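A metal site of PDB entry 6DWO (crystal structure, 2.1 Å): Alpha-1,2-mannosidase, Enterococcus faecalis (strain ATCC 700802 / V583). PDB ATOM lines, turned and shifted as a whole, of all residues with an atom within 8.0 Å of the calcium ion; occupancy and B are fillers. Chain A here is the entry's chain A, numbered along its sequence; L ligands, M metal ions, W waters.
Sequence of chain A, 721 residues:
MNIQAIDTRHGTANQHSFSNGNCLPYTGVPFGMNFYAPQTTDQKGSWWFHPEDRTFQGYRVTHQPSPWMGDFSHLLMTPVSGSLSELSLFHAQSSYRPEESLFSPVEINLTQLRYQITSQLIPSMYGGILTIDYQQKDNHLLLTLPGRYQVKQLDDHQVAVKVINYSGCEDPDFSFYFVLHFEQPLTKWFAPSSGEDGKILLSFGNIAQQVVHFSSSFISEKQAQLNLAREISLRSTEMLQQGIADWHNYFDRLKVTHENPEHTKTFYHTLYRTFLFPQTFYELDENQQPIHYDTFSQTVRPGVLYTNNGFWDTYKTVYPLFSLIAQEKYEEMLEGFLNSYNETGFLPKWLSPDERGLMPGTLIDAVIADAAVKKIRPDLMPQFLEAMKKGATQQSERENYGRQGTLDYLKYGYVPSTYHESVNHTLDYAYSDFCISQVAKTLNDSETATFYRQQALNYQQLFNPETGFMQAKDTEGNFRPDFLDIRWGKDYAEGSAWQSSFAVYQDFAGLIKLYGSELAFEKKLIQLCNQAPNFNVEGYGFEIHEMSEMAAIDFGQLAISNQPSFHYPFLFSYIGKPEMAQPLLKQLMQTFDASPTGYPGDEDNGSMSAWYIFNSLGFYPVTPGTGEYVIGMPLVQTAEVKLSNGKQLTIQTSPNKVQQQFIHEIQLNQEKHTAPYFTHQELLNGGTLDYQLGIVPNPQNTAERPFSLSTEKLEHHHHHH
Water W2 bridges O of Ser 561 and O of Asp 602.
The side-chain carboxylate of Asp 313 sits close to the side-chain amide oxygen of Gln 563, at 3.4 Å. The side-chain amide nitrogen (NE2) of Gln 563 sits at hydrogen-bond distance from the side-chain hydroxyl (OG) of Ser 607 (3.1 Å). The side-chain amide nitrogen of Asn 562 sits at hydrogen-bond distance from the side-chain carboxylate of Glu 494.
Three residues have an atom within 4 Å of the calcium ion: Asn 562, Gln 563 and Asp 604. The nearest printed residue that does not touch the calcium ion is Asp 602 (4.1 Å).
The calcium ion is bound by OD2 of Asp 604, 2.4 Å away. OE1 of Gln 563 binds the calcium ion. The calcium ion is bound by O3 of the ligand, 2.5 Å away. The calcium ion is bound by water W2 (2.6 Å). The calcium ion is bound by the side-chain amide oxygen (OD1) of Asn 562 (2.6 Å). The calcium ion is bound by water W1. The calcium ion has six donor atoms within binding distance.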
ATOM      1  N   TRP A  68      16.658  17.803 -21.446  1.00  0.00           N
ATOM      2  CA  TRP A  68      17.230  18.439 -20.266  1.00  0.00           C
ATOM      3  C   TRP A  68      16.779  19.896 -20.199  1.00  0.00           C
ATOM      4  O   TRP A  68      16.680  20.443 -19.105  1.00  0.00           O
ATOM      5  CB  TRP A  68      18.765  18.310 -20.208  1.00  0.00           C
ATOM      6  CG  TRP A  68      19.180  16.889 -20.436  1.00  0.00           C
ATOM      7  CD1 TRP A  68      19.811  16.385 -21.545  1.00  0.00           C
ATOM      8  CD2 TRP A  68      18.945  15.771 -19.557  1.00  0.00           C
ATOM      9  NE1 TRP A  68      19.953  15.029 -21.416  1.00  0.00           N
ATOM     10  CE2 TRP A  68      19.434  14.617 -20.216  1.00  0.00           C
ATOM     11  CE3 TRP A  68      18.371  15.626 -18.280  1.00  0.00           C
ATOM     12  CZ2 TRP A  68      19.384  13.339 -19.635  1.00  0.00           C
ATOM     13  CZ3 TRP A  68      18.300  14.369 -17.708  1.00  0.00           C
ATOM     14  CH2 TRP A  68      18.815  13.237 -18.384  1.00  0.00           C
ATOM     15  N   TRP A 312      28.456  25.495 -25.381  1.00  0.00           N
ATOM     16  CA  TRP A 312      29.323  24.512 -24.772  1.00  0.00           C
ATOM     17  C   TRP A 312      29.363  23.245 -25.627  1.00  0.00           C
ATOM     18  O   TRP A 312      30.396  22.589 -25.718  1.00  0.00           O
ATOM     19  CB  TRP A 312      28.824  24.239 -23.344  1.00  0.00           C
ATOM     20  CG  TRP A 312      29.678  23.341 -22.485  1.00  0.00           C
ATOM     21  CD1 TRP A 312      30.658  23.742 -21.624  1.00  0.00           C
ATOM     22  CD2 TRP A 312      29.593  21.904 -22.360  1.00  0.00           C
ATOM     23  NE1 TRP A 312      31.179  22.659 -20.959  1.00  0.00           N
ATOM     24  CE2 TRP A 312      30.549  21.518 -21.380  1.00  0.00           C
ATOM     25  CE3 TRP A 312      28.821  20.898 -22.955  1.00  0.00           C
ATOM     26  CZ2 TRP A 312      30.746  20.182 -21.016  1.00  0.00           C
ATOM     27  CZ3 TRP A 312      29.006  19.574 -22.592  1.00  0.00           C
ATOM     28  CH2 TRP A 312      29.979  19.218 -21.638  1.00  0.00           C
ATOM     29  N   ASP A 313      28.236  22.918 -26.283  1.00  0.00           N
ATOM     30  CA  ASP A 313      28.137  21.765 -27.154  1.00  0.00           C
ATOM     31  C   ASP A 313      28.515  22.146 -28.584  1.00  0.00           C
ATOM     32  O   ASP A 313      29.284  21.451 -29.248  1.00  0.00           O
ATOM     33  CB  ASP A 313      26.695  21.256 -27.268  1.00  0.00           C
ATOM     34  CG  ASP A 313      26.085  20.826 -25.944  1.00  0.00           C
ATOM     35  OD1 ASP A 313      26.842  20.134 -25.155  1.00  0.00           O
ATOM     36  OD2 ASP A 313      24.864  21.201 -25.676  1.00  0.00           O
ATOM     37  N   MET A 359      25.483  24.980 -18.051  1.00  0.00           N
ATOM     38  CA  MET A 359      26.797  24.459 -18.422  1.00  0.00           C
ATOM     39  C   MET A 359      27.866  25.486 -18.060  1.00  0.00           C
ATOM     40  O   MET A 359      27.607  26.687 -17.985  1.00  0.00           O
ATOM     41  CB  MET A 359      26.914  24.050 -19.900  1.00  0.00           C
ATOM     42  CG  MET A 359      25.911  22.953 -20.325  1.00  0.00           C
ATOM     43  SD  MET A 359      25.910  21.497 -19.220  1.00  0.00           S
ATOM     44  CE  MET A 359      24.185  20.989 -19.199  1.00  0.00           C
ATOM     45  N   GLU A 494      29.965  16.254 -15.615  1.00  0.00           N
ATOM     46  CA  GLU A 494      29.591  15.102 -16.424  1.00  0.00           C
ATOM     47  C   GLU A 494      30.836  14.295 -16.831  1.00  0.00           C
ATOM     48  O   GLU A 494      30.964  13.874 -17.983  1.00  0.00           O
ATOM     49  CB  GLU A 494      28.861  15.588 -17.674  1.00  0.00           C
ATOM     50  CG  GLU A 494      27.590  16.374 -17.383  1.00  0.00           C
ATOM     51  CD  GLU A 494      26.939  16.884 -18.674  1.00  0.00           C
ATOM     52  OE1 GLU A 494      25.786  17.380 -18.637  1.00  0.00           O
ATOM     53  OE2 GLU A 494      27.586  16.807 -19.740  1.00  0.00           O
ATOM     54  N   HIS A 545      23.410   9.017 -16.707  1.00  0.00           N
ATOM     55  CA  HIS A 545      23.414   8.380 -18.022  1.00  0.00           C
ATOM     56  C   HIS A 545      24.790   8.473 -18.688  1.00  0.00           C
ATOM     57  O   HIS A 545      25.201   7.516 -19.350  1.00  0.00           O
ATOM     58  CB  HIS A 545      22.245   8.862 -18.909  1.00  0.00           C
ATOM     59  CG  HIS A 545      22.400  10.273 -19.387  1.00  0.00           C
ATOM     60  ND1 HIS A 545      22.901  10.556 -20.664  1.00  0.00           N
ATOM     61  CD2 HIS A 545      22.118  11.466 -18.796  1.00  0.00           C
ATOM     62  CE1 HIS A 545      22.911  11.869 -20.833  1.00  0.00           C
ATOM     63  NE2 HIS A 545      22.413  12.462 -19.706  1.00  0.00           N
ATOM     64  N   GLU A 546      25.528   9.566 -18.494  1.00  0.00           N
ATOM     65  CA  GLU A 546      26.823   9.728 -19.142  1.00  0.00           C
ATOM     66  C   GLU A 546      27.812   8.655 -18.673  1.00  0.00           C
ATOM     67  O   GLU A 546      28.659   8.215 -19.446  1.00  0.00           O
ATOM     68  CB  GLU A 546      27.440  11.097 -18.870  1.00  0.00           C
ATOM     69  CG  GLU A 546      26.800  12.212 -19.680  1.00  0.00           C
ATOM     70  CD  GLU A 546      25.632  12.888 -18.990  1.00  0.00           C
ATOM     71  OE1 GLU A 546      25.169  13.955 -19.498  1.00  0.00           O
ATOM     72  OE2 GLU A 546      25.158  12.352 -17.945  1.00  0.00           O
ATOM     73  N   GLU A 549      26.742   5.353 -20.439  1.00  0.00           N
ATOM     74  CA  GLU A 549      27.005   5.337 -21.864  1.00  0.00           C
ATOM     75  C   GLU A 549      28.494   5.046 -22.097  1.00  0.00           C
ATOM     76  O   GLU A 549      28.804   4.312 -23.011  1.00  0.00           O
ATOM     77  CB  GLU A 549      26.555   6.659 -22.512  1.00  0.00           C
ATOM     78  CG  GLU A 549      25.056   6.817 -22.534  1.00  0.00           C
ATOM     79  CD  GLU A 549      24.606   8.240 -22.272  1.00  0.00           C
ATOM     80  OE1 GLU A 549      25.428   9.201 -22.430  1.00  0.00           O
ATOM     81  OE2 GLU A 549      23.425   8.387 -21.868  1.00  0.00           O
ATOM     82  N   ILE A 560      33.096   8.954 -25.741  1.00  0.00           N
ATOM     83  CA  ILE A 560      32.637   9.580 -26.978  1.00  0.00           C
ATOM     84  C   ILE A 560      31.155   9.972 -26.849  1.00  0.00           C
ATOM     85  O   ILE A 560      30.649  10.759 -27.645  1.00  0.00           O
ATOM     86  CB  ILE A 560      32.894   8.630 -28.177  1.00  0.00           C
ATOM     87  CG1 ILE A 560      32.619   9.292 -29.531  1.00  0.00           C
ATOM     88  CG2 ILE A 560      32.156   7.300 -28.027  1.00  0.00           C
ATOM     89  CD1 ILE A 560      33.524  10.496 -29.813  1.00  0.00           C
ATOM     90  N   SER A 561      30.457   9.407 -25.856  1.00  0.00           N
ATOM     91  CA  SER A 561      29.061   9.713 -25.562  1.00  0.00           C
ATOM     92  C   SER A 561      28.883  11.169 -25.098  1.00  0.00           C
ATOM     93  O   SER A 561      27.756  11.649 -24.986  1.00  0.00           O
ATOM     94  CB  SER A 561      28.564   8.755 -24.515  1.00  0.00           C
ATOM     95  OG  SER A 561      29.468   8.715 -23.406  1.00  0.00           O
ATOM     96  N   ASN A 562      29.980  11.886 -24.812  1.00  0.00           N
ATOM     97  CA  ASN A 562      29.859  13.248 -24.296  1.00  0.00           C
ATOM     98  C   ASN A 562      30.951  14.142 -24.889  1.00  0.00           C
ATOM     99  O   ASN A 562      32.052  13.682 -25.185  1.00  0.00           O
ATOM    100  CB  ASN A 562      29.901  13.247 -22.761  1.00  0.00           C
ATOM    101  CG  ASN A 562      29.264  14.480 -22.137  1.00  0.00           C
ATOM    102  OD1 ASN A 562      28.521  15.200 -22.782  1.00  0.00           O
ATOM    103  ND2 ASN A 562      29.547  14.721 -20.870  1.00  0.00           N
ATOM    104  N   GLN A 563      30.641  15.453 -24.992  1.00  0.00           N
ATOM    105  CA  GLN A 563      31.454  16.426 -25.723  1.00  0.00           C
ATOM    106  C   GLN A 563      32.898  16.536 -25.220  1.00  0.00           C
ATOM    107  O   GLN A 563      33.809  16.771 -26.016  1.00  0.00           O
ATOM    108  CB  GLN A 563      30.790  17.817 -25.728  1.00  0.00           C
ATOM    109  CG  GLN A 563      29.711  17.963 -26.814  1.00  0.00           C
ATOM    110  CD  GLN A 563      28.433  17.347 -26.305  1.00  0.00           C
ATOM    111  OE1 GLN A 563      28.293  17.007 -25.125  1.00  0.00           O
ATOM    112  NE2 GLN A 563      27.466  17.197 -27.199  1.00  0.00           N
ATOM    113  N   PRO A 564      33.175  16.450 -23.891  1.00  0.00           N
ATOM    114  CA  PRO A 564      34.543  16.629 -23.407  1.00  0.00           C
ATOM    115  C   PRO A 564      35.580  15.699 -24.015  1.00  0.00           C
ATOM    116  O   PRO A 564      36.754  16.064 -24.052  1.00  0.00           O
ATOM    117  CB  PRO A 564      34.387  16.348 -21.884  1.00  0.00           C
ATOM    118  CG  PRO A 564      32.960  16.871 -21.609  1.00  0.00           C
ATOM    119  CD  PRO A 564      32.207  16.303 -22.792  1.00  0.00           C
ATOM    120  N   PHE A 566      35.486  14.487 -27.216  1.00  0.00           N
ATOM    121  CA  PHE A 566      35.360  14.465 -28.672  1.00  0.00           C
ATOM    122  C   PHE A 566      36.729  14.573 -29.352  1.00  0.00           C
ATOM    123  O   PHE A 566      36.930  13.975 -30.413  1.00  0.00           O
ATOM    124  CB  PHE A 566      34.468  15.593 -29.184  1.00  0.00           C
ATOM    125  CG  PHE A 566      32.983  15.335 -29.190  1.00  0.00           C
ATOM    126  CD1 PHE A 566      32.444  14.250 -28.509  1.00  0.00           C
ATOM    127  CD2 PHE A 566      32.120  16.214 -29.832  1.00  0.00           C
ATOM    128  CE1 PHE A 566      31.065  14.046 -28.499  1.00  0.00           C
ATOM    129  CE2 PHE A 566      30.741  16.011 -29.822  1.00  0.00           C
ATOM    130  CZ  PHE A 566      30.221  14.928 -29.134  1.00  0.00           C
ATOM    131  N   GLY A 601      25.636   8.720 -27.389  1.00  0.00           N
ATOM    132  CA  GLY A 601      25.177   9.549 -26.273  1.00  0.00           C
ATOM    133  C   GLY A 601      24.341  10.729 -26.806  1.00  0.00           C
ATOM    134  O   GLY A 601      23.934  10.709 -27.970  1.00  0.00           O
ATOM    135  N   ASP A 602      24.163  11.772 -25.997  1.00  0.00           N
ATOM    136  CA  ASP A 602      23.302  12.891 -26.422  1.00  0.00           C
ATOM    137  C   ASP A 602      23.838  13.579 -27.670  1.00  0.00           C
ATOM    138  O   ASP A 602      25.012  13.974 -27.715  1.00  0.00           O
ATOM    139  CB  ASP A 602      23.210  13.942 -25.316  1.00  0.00           C
ATOM    140  CG  ASP A 602      22.258  13.540 -24.205  1.00  0.00           C
ATOM    141  OD1 ASP A 602      21.749  12.390 -24.196  1.00  0.00           O
ATOM    142  OD2 ASP A 602      22.036  14.368 -23.350  1.00  0.00           O
ATOM    143  N   GLU A 603      22.968  13.766 -28.667  1.00  0.00           N
ATOM    144  CA  GLU A 603      23.353  14.362 -29.940  1.00  0.00           C
ATOM    145  C   GLU A 603      23.617  15.872 -29.779  1.00  0.00           C
ATOM    146  O   GLU A 603      24.494  16.431 -30.459  1.00  0.00           O
ATOM    147  CB  GLU A 603      22.248  14.059 -30.954  1.00  0.00           C
ATOM    148  CG  GLU A 603      22.651  14.359 -32.395  1.00  0.00           C
ATOM    149  CD  GLU A 603      22.616  15.832 -32.773  1.00  0.00           C
ATOM    150  OE1 GLU A 603      21.712  16.581 -32.277  1.00  0.00           O
ATOM    151  OE2 GLU A 603      23.516  16.259 -33.548  1.00  0.00           O
ATOM    152  N   ASP A 604      22.815  16.547 -28.922  1.00  0.00           N
ATOM    153  CA  ASP A 604      22.995  17.943 -28.542  1.00  0.00           C
ATOM    154  C   ASP A 604      23.058  18.914 -29.731  1.00  0.00           C
ATOM    155  O   ASP A 604      24.075  19.548 -29.976  1.00  0.00           O
ATOM    156  CB  ASP A 604      24.224  18.137 -27.641  1.00  0.00           C
ATOM    157  CG  ASP A 604      24.065  17.494 -26.265  1.00  0.00           C
ATOM    158  OD1 ASP A 604      22.962  17.603 -25.640  1.00  0.00           O
ATOM    159  OD2 ASP A 604      25.026  16.840 -25.832  1.00  0.00           O
ATOM    160  N   SER A 607      25.771  18.873 -32.508  1.00  0.00           N
ATOM    161  CA  SER A 607      27.101  18.760 -31.948  1.00  0.00           C
ATOM    162  C   SER A 607      27.745  17.410 -32.282  1.00  0.00           C
ATOM    163  O   SER A 607      28.822  17.313 -32.874  1.00  0.00           O
ATOM    164  CB  SER A 607      26.957  18.920 -30.458  1.00  0.00           C
ATOM    165  OG  SER A 607      28.194  18.774 -29.817  1.00  0.00           O
ATOM    166  N   MET A 608      27.067  16.322 -31.901  1.00  0.00           N
ATOM    167  CA  MET A 608      27.586  14.983 -32.146  1.00  0.00           C
ATOM    168  C   MET A 608      27.464  14.609 -33.635  1.00  0.00           C
ATOM    169  O   MET A 608      28.306  13.864 -34.138  1.00  0.00           O
ATOM    170  CB  MET A 608      26.912  13.951 -31.254  1.00  0.00           C
ATOM    171  CG  MET A 608      27.654  12.606 -31.216  1.00  0.00           C
ATOM    172  SD  MET A 608      26.835  11.509 -29.999  1.00  0.00           S
ATOM    173  CE  MET A 608      27.561  12.051 -28.445  1.00  0.00           C
HETATM  174  C1  LIG L   1      24.660  20.779 -22.672  1.00  0.00           C
HETATM  175  O1  LIG L   1      23.381  21.210 -23.109  1.00  0.00           O
HETATM  176  C2  LIG L   1      24.556  19.312 -22.275  1.00  0.00           C
HETATM  177  O2  LIG L   1      24.150  18.490 -23.377  1.00  0.00           O
HETATM  178  C3  LIG L   1      25.910  18.863 -21.776  1.00  0.00           C
HETATM  179  O3  LIG L   1      26.051  17.441 -21.811  1.00  0.00           O
HETATM  180 CA    CA M   1      26.367  16.114 -23.950  1.00  0.00          CA
HETATM  181  O   HOH W   1      25.371  14.234 -22.236  1.00  0.00           O
HETATM  182  O   HOH W   2      26.691  14.015 -25.406  1.00  0.00           O
